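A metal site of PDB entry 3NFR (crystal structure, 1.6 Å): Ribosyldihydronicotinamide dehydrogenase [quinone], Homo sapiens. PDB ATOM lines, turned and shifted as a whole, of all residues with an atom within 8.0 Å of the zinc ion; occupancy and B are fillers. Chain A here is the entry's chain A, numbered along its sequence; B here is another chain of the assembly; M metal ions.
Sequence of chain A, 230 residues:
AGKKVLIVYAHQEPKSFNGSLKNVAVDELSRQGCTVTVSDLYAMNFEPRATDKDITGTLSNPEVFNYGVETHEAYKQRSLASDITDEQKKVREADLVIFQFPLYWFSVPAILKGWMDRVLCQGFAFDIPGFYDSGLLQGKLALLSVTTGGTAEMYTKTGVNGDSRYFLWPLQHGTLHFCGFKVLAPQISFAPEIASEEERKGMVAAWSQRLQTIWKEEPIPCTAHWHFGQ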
ATOM      1  N   TYR A 132     -21.998 -15.583  12.643  1.00  0.00           N
ATOM      2  CA  TYR A 132     -23.312 -16.017  12.161  1.00  0.00           C
ATOM      3  C   TYR A 132     -23.769 -15.317  10.842  1.00  0.00           C
ATOM      4  O   TYR A 132     -23.023 -15.382   9.846  1.00  0.00           O
ATOM      5  CB  TYR A 132     -24.348 -15.972  13.307  1.00  0.00           C
ATOM      6  CG  TYR A 132     -23.984 -17.057  14.331  1.00  0.00           C
ATOM      7  CD1 TYR A 132     -23.936 -18.401  13.930  1.00  0.00           C
ATOM      8  CD2 TYR A 132     -23.643 -16.729  15.664  1.00  0.00           C
ATOM      9  CE1 TYR A 132     -23.594 -19.410  14.853  1.00  0.00           C
ATOM     10  CE2 TYR A 132     -23.332 -17.746  16.613  1.00  0.00           C
ATOM     11  CZ  TYR A 132     -23.319 -19.073  16.162  1.00  0.00           C
ATOM     12  OH  TYR A 132     -22.951 -20.077  17.026  1.00  0.00           O
ATOM     13  N   ASP A 133     -24.957 -14.699  10.813  1.00  0.00           N
ATOM     14  CA  ASP A 133     -25.391 -13.950   9.631  1.00  0.00           C
ATOM     15  C   ASP A 133     -24.361 -12.943   9.089  1.00  0.00           C
ATOM     16  O   ASP A 133     -24.331 -12.616   7.861  1.00  0.00           O
ATOM     17  CB  ASP A 133     -26.699 -13.244   9.991  1.00  0.00           C
ATOM     18  CG  ASP A 133     -27.856 -14.193   9.939  1.00  0.00           C
ATOM     19  OD1 ASP A 133     -27.550 -15.413   9.790  1.00  0.00           O
ATOM     20  OD2 ASP A 133     -29.040 -13.768  10.002  1.00  0.00           O
ATOM     21  N   TRP A 169     -25.629 -29.847  13.852  1.00  0.00           N
ATOM     22  CA  TRP A 169     -25.484 -28.627  14.534  1.00  0.00           C
ATOM     23  C   TRP A 169     -24.070 -28.073  14.652  1.00  0.00           C
ATOM     24  O   TRP A 169     -23.842 -26.908  14.311  1.00  0.00           O
ATOM     25  CB  TRP A 169     -26.198 -28.746  15.917  1.00  0.00           C
ATOM     26  CG  TRP A 169     -26.093 -27.547  16.827  1.00  0.00           C
ATOM     27  CD1 TRP A 169     -25.349 -27.442  17.994  1.00  0.00           C
ATOM     28  CD2 TRP A 169     -26.811 -26.297  16.732  1.00  0.00           C
ATOM     29  NE1 TRP A 169     -25.520 -26.206  18.597  1.00  0.00           N
ATOM     30  CE2 TRP A 169     -26.441 -25.493  17.846  1.00  0.00           C
ATOM     31  CE3 TRP A 169     -27.740 -25.764  15.790  1.00  0.00           C
ATOM     32  CZ2 TRP A 169     -26.932 -24.166  18.050  1.00  0.00           C
ATOM     33  CZ3 TRP A 169     -28.226 -24.463  15.985  1.00  0.00           C
ATOM     34  CH2 TRP A 169     -27.846 -23.694  17.140  1.00  0.00           C
ATOM     35  N   LEU A 171     -21.560 -28.644  12.923  1.00  0.00           N
ATOM     36  CA  LEU A 171     -20.976 -28.435  11.545  1.00  0.00           C
ATOM     37  C   LEU A 171     -21.705 -27.298  10.808  1.00  0.00           C
ATOM     38  O   LEU A 171     -21.043 -26.310  10.490  1.00  0.00           O
ATOM     39  CB  LEU A 171     -21.025 -29.728  10.722  1.00  0.00           C
ATOM     40  CG  LEU A 171     -20.134 -30.853  11.336  1.00  0.00           C
ATOM     41  CD1 LEU A 171     -20.572 -32.106  10.664  1.00  0.00           C
ATOM     42  CD2 LEU A 171     -18.592 -30.523  11.239  1.00  0.00           C
ATOM     43  N   GLN A 172     -23.002 -27.472  10.667  1.00  0.00           N
ATOM     44  CA  GLN A 172     -23.778 -26.421   9.992  1.00  0.00           C
ATOM     45  C   GLN A 172     -23.838 -25.146  10.751  1.00  0.00           C
ATOM     46  O   GLN A 172     -23.600 -24.038  10.186  1.00  0.00           O
ATOM     47  CB  GLN A 172     -25.127 -26.947   9.727  1.00  0.00           C
ATOM     48  CG  GLN A 172     -25.110 -27.942   8.601  1.00  0.00           C
ATOM     49  CD  GLN A 172     -26.488 -28.331   8.169  1.00  0.00           C
ATOM     50  OE1 GLN A 172     -27.467 -28.188   8.967  1.00  0.00           O
ATOM     51  NE2 GLN A 172     -26.605 -28.993   7.036  1.00  0.00           N
ATOM     52  N   HIS A 173     -24.206 -25.216  12.052  1.00  0.00           N
ATOM     53  CA  HIS A 173     -24.340 -23.972  12.852  1.00  0.00           C
ATOM     54  C   HIS A 173     -23.085 -23.458  13.437  1.00  0.00           C
ATOM     55  O   HIS A 173     -22.658 -22.337  13.195  1.00  0.00           O
ATOM     56  CB  HIS A 173     -25.445 -24.128  13.956  1.00  0.00           C
ATOM     57  CG  HIS A 173     -25.731 -22.838  14.678  1.00  0.00           C
ATOM     58  ND1 HIS A 173     -26.495 -21.836  14.125  1.00  0.00           N
ATOM     59  CD2 HIS A 173     -25.335 -22.373  15.899  1.00  0.00           C
ATOM     60  CE1 HIS A 173     -26.543 -20.802  14.948  1.00  0.00           C
ATOM     61  NE2 HIS A 173     -25.863 -21.109  16.040  1.00  0.00           N
ATOM     62  N   GLY A 174     -22.403 -24.293  14.243  1.00  0.00           N
ATOM     63  CA  GLY A 174     -21.258 -23.828  14.980  1.00  0.00           C
ATOM     64  C   GLY A 174     -20.058 -23.550  14.093  1.00  0.00           C
ATOM     65  O   GLY A 174     -19.177 -22.854  14.523  1.00  0.00           O
ATOM     66  N   THR A 175     -20.073 -24.134  12.893  1.00  0.00           N
ATOM     67  CA  THR A 175     -18.891 -23.893  12.011  1.00  0.00           C
ATOM     68  C   THR A 175     -19.346 -23.119  10.745  1.00  0.00           C
ATOM     69  O   THR A 175     -18.861 -21.994  10.639  1.00  0.00           O
ATOM     70  CB  THR A 175     -18.209 -25.213  11.611  1.00  0.00           C
ATOM     71  OG1 THR A 175     -17.905 -25.934  12.823  1.00  0.00           O
ATOM     72  CG2 THR A 175     -16.875 -24.938  10.905  1.00  0.00           C
ATOM     73  N   LEU A 176     -20.254 -23.672   9.935  1.00  0.00           N
ATOM     74  CA  LEU A 176     -20.494 -22.955   8.557  1.00  0.00           C
ATOM     75  C   LEU A 176     -21.223 -21.611   8.750  1.00  0.00           C
ATOM     76  O   LEU A 176     -20.668 -20.573   8.462  1.00  0.00           O
ATOM     77  CB  LEU A 176     -21.133 -23.871   7.562  1.00  0.00           C
ATOM     78  CG  LEU A 176     -20.195 -25.128   7.343  1.00  0.00           C
ATOM     79  CD1 LEU A 176     -21.029 -26.138   6.593  1.00  0.00           C
ATOM     80  CD2 LEU A 176     -18.912 -24.732   6.675  1.00  0.00           C
ATOM     81  N   HIS A 177     -22.364 -21.660   9.444  1.00  0.00           N
ATOM     82  CA  HIS A 177     -23.122 -20.400   9.769  1.00  0.00           C
ATOM     83  C   HIS A 177     -22.290 -19.422  10.500  1.00  0.00           C
ATOM     84  O   HIS A 177     -22.266 -18.194  10.259  1.00  0.00           O
ATOM     85  CB  HIS A 177     -24.389 -20.764  10.551  1.00  0.00           C
ATOM     86  CG  HIS A 177     -25.337 -19.601  10.722  1.00  0.00           C
ATOM     87  ND1 HIS A 177     -26.581 -19.757  11.281  1.00  0.00           N
ATOM     88  CD2 HIS A 177     -25.245 -18.309  10.323  1.00  0.00           C
ATOM     89  CE1 HIS A 177     -27.216 -18.594  11.269  1.00  0.00           C
ATOM     90  NE2 HIS A 177     -26.434 -17.700  10.689  1.00  0.00           N
ATOM     91  N   PHE A 178     -21.550 -19.878  11.468  1.00  0.00           N
ATOM     92  CA  PHE A 178     -20.726 -19.058  12.186  1.00  0.00           C
ATOM     93  C   PHE A 178     -19.777 -18.218  11.346  1.00  0.00           C
ATOM     94  O   PHE A 178     -19.589 -17.080  11.595  1.00  0.00           O
ATOM     95  CB  PHE A 178     -19.969 -19.863  13.282  1.00  0.00           C
ATOM     96  CG  PHE A 178     -19.203 -19.000  14.187  1.00  0.00           C
ATOM     97  CD1 PHE A 178     -19.866 -18.494  15.380  1.00  0.00           C
ATOM     98  CD2 PHE A 178     -17.935 -18.628  13.987  1.00  0.00           C
ATOM     99  CE1 PHE A 178     -19.179 -17.665  16.283  1.00  0.00           C
ATOM    100  CE2 PHE A 178     -17.220 -17.815  14.804  1.00  0.00           C
ATOM    101  CZ  PHE A 178     -17.856 -17.249  16.040  1.00  0.00           C
ATOM    102  N   PHE A 181     -21.403 -18.486   6.037  1.00  0.00           N
ATOM    103  CA  PHE A 181     -22.072 -19.252   5.030  1.00  0.00           C
ATOM    104  C   PHE A 181     -23.582 -19.355   5.134  1.00  0.00           C
ATOM    105  O   PHE A 181     -24.154 -19.596   6.200  1.00  0.00           O
ATOM    106  CB  PHE A 181     -21.543 -20.730   4.975  1.00  0.00           C
ATOM    107  CG  PHE A 181     -20.088 -20.901   4.546  1.00  0.00           C
ATOM    108  CD1 PHE A 181     -19.731 -20.948   3.201  1.00  0.00           C
ATOM    109  CD2 PHE A 181     -19.086 -21.181   5.470  1.00  0.00           C
ATOM    110  CE1 PHE A 181     -18.373 -21.181   2.798  1.00  0.00           C
ATOM    111  CE2 PHE A 181     -17.753 -21.439   5.099  1.00  0.00           C
ATOM    112  CZ  PHE A 181     -17.426 -21.436   3.701  1.00  0.00           C
ATOM    113  N   VAL A 183     -26.082 -22.064   4.405  1.00  0.00           N
ATOM    114  CA  VAL A 183     -26.064 -23.478   4.290  1.00  0.00           C
ATOM    115  C   VAL A 183     -27.159 -24.057   3.476  1.00  0.00           C
ATOM    116  O   VAL A 183     -28.383 -23.972   3.844  1.00  0.00           O
ATOM    117  CB  VAL A 183     -26.082 -24.141   5.737  1.00  0.00           C
ATOM    118  CG1 VAL A 183     -25.865 -25.647   5.729  1.00  0.00           C
ATOM    119  CG2 VAL A 183     -25.157 -23.479   6.619  1.00  0.00           C
ATOM    120  N   ILE A 220     -31.187 -23.214   3.922  1.00  0.00           N
ATOM    121  CA  ILE A 220     -31.970 -23.533   5.112  1.00  0.00           C
ATOM    122  C   ILE A 220     -31.913 -22.393   6.134  1.00  0.00           C
ATOM    123  O   ILE A 220     -30.980 -21.596   6.143  1.00  0.00           O
ATOM    124  CB  ILE A 220     -31.511 -24.870   5.759  1.00  0.00           C
ATOM    125  CG1 ILE A 220     -30.073 -24.782   6.301  1.00  0.00           C
ATOM    126  CG2 ILE A 220     -31.678 -25.997   4.778  1.00  0.00           C
ATOM    127  CD1 ILE A 220     -29.687 -25.826   7.439  1.00  0.00           C
ATOM    128  N   PRO A 221     -32.952 -22.291   6.988  1.00  0.00           N
ATOM    129  CA  PRO A 221     -32.831 -21.399   8.146  1.00  0.00           C
ATOM    130  C   PRO A 221     -31.909 -22.080   9.153  1.00  0.00           C
ATOM    131  O   PRO A 221     -32.311 -23.138   9.665  1.00  0.00           O
ATOM    132  CB  PRO A 221     -34.254 -21.378   8.737  1.00  0.00           C
ATOM    133  CG  PRO A 221     -34.993 -22.537   8.123  1.00  0.00           C
ATOM    134  CD  PRO A 221     -34.318 -22.804   6.784  1.00  0.00           C
ATOM    135  N   CYS A 222     -30.693 -21.534   9.360  1.00  0.00           N
ATOM    136  CA  CYS A 222     -29.675 -22.267  10.167  1.00  0.00           C
ATOM    137  C   CYS A 222     -29.915 -21.919  11.627  1.00  0.00           C
ATOM    138  O   CYS A 222     -29.174 -21.113  12.221  1.00  0.00           O
ATOM    139  CB  CYS A 222     -28.222 -21.964   9.741  1.00  0.00           C
ATOM    140  SG  CYS A 222     -26.964 -23.072  10.634  1.00  0.00           S
ATOM    141  N   THR A 223     -30.990 -22.488  12.118  1.00  0.00           N
ATOM    142  CA  THR A 223     -31.450 -22.155  13.477  1.00  0.00           C
ATOM    143  C   THR A 223     -31.503 -23.347  14.399  1.00  0.00           C
ATOM    144  O   THR A 223     -31.614 -24.508  13.984  1.00  0.00           O
ATOM    145  CB  THR A 223     -32.890 -21.465  13.446  1.00  0.00           C
ATOM    146  OG1 THR A 223     -33.862 -22.392  12.958  1.00  0.00           O
ATOM    147  CG2 THR A 223     -32.867 -20.163  12.628  1.00  0.00           C
ATOM    148  N   ALA A 224     -31.476 -23.033  15.697  1.00  0.00           N
ATOM    149  CA  ALA A 224     -31.683 -24.040  16.734  1.00  0.00           C
ATOM    150  C   ALA A 224     -33.036 -24.717  16.458  1.00  0.00           C
ATOM    151  O   ALA A 224     -33.144 -25.931  16.476  1.00  0.00           O
ATOM    152  CB  ALA A 224     -31.596 -23.383  18.185  1.00  0.00           C
ATOM    153  N   TRP A 226     -34.518 -25.137  13.449  1.00  0.00           N
ATOM    154  CA  TRP A 226     -34.383 -26.073  12.322  1.00  0.00           C
ATOM    155  C   TRP A 226     -33.735 -27.394  12.788  1.00  0.00           C
ATOM    156  O   TRP A 226     -34.136 -28.521  12.390  1.00  0.00           O
ATOM    157  CB  TRP A 226     -33.557 -25.429  11.154  1.00  0.00           C
ATOM    158  CG  TRP A 226     -33.513 -26.288   9.879  1.00  0.00           C
ATOM    159  CD1 TRP A 226     -34.414 -26.267   8.842  1.00  0.00           C
ATOM    160  CD2 TRP A 226     -32.565 -27.323   9.564  1.00  0.00           C
ATOM    161  NE1 TRP A 226     -34.094 -27.226   7.899  1.00  0.00           N
ATOM    162  CE2 TRP A 226     -32.936 -27.868   8.303  1.00  0.00           C
ATOM    163  CE3 TRP A 226     -31.414 -27.832  10.212  1.00  0.00           C
ATOM    164  CZ2 TRP A 226     -32.207 -28.912   7.674  1.00  0.00           C
ATOM    165  CZ3 TRP A 226     -30.693 -28.885   9.604  1.00  0.00           C
ATOM    166  CH2 TRP A 226     -31.086 -29.405   8.345  1.00  0.00           C
ATOM    167  N   HIS A 227     -32.712 -27.262  13.648  1.00  0.00           N
ATOM    168  CA  HIS A 227     -31.990 -28.450  14.114  1.00  0.00           C
ATOM    169  C   HIS A 227     -32.722 -29.321  15.138  1.00  0.00           C
ATOM    170  O   HIS A 227     -32.689 -30.547  15.044  1.00  0.00           O
ATOM    171  CB  HIS A 227     -30.599 -28.068  14.615  1.00  0.00           C
ATOM    172  CG  HIS A 227     -29.674 -27.624  13.513  1.00  0.00           C
ATOM    173  ND1 HIS A 227     -29.670 -26.316  13.055  1.00  0.00           N
ATOM    174  CD2 HIS A 227     -28.783 -28.312  12.768  1.00  0.00           C
ATOM    175  CE1 HIS A 227     -28.745 -26.212  12.087  1.00  0.00           C
ATOM    176  NE2 HIS A 227     -28.205 -27.416  11.896  1.00  0.00           N
ATOM    177  N   VAL B 160     -26.714 -17.063  21.334  1.00  0.00           N
ATOM    178  CA  VAL B 160     -26.289 -17.177  19.920  1.00  0.00           C
ATOM    179  C   VAL B 160     -25.841 -18.586  19.573  1.00  0.00           C
ATOM    180  O   VAL B 160     -26.230 -19.212  18.528  1.00  0.00           O
ATOM    181  CB  VAL B 160     -25.022 -16.323  19.746  1.00  0.00           C
ATOM    182  CG1 VAL B 160     -25.251 -15.125  18.840  1.00  0.00           C
ATOM    183  CG2 VAL B 160     -24.452 -15.925  21.096  1.00  0.00           C
HETATM  184 ZN    ZN M   1     -27.074 -21.569  12.149  1.00  0.00          ZN
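The zinc ion is bound by ND1 of His 177 (2.1 Å), ND1 of His 173 (2.1 Å), SG of Cys 222 (2.1 Å) and O of Cys 222 (2.2 Å). The zinc ion has four donor atoms within binding distance.
O of Gln 172 sits close to SG of Cys 222 (3.5 Å). A ring nitrogen (NE2) of His 173 sits close to the side-chain hydroxyl of Tyr 132, at 3.2 Å. O of Gln 172 is in hydrogen-bond range of N of His 177. NE2 of His 177 lies within hydrogen-bond range of OD1 of Asp 133. NE2 of His 173 is in hydrogen-bond range of O of Val 160 of chain B (3.2 Å). O of His 173 is in hydrogen-bond range of N of Phe 178, 3.2 Å away.
The nearest printed residue that does not touch the zinc ion is Thr 223 (4.02 Å).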
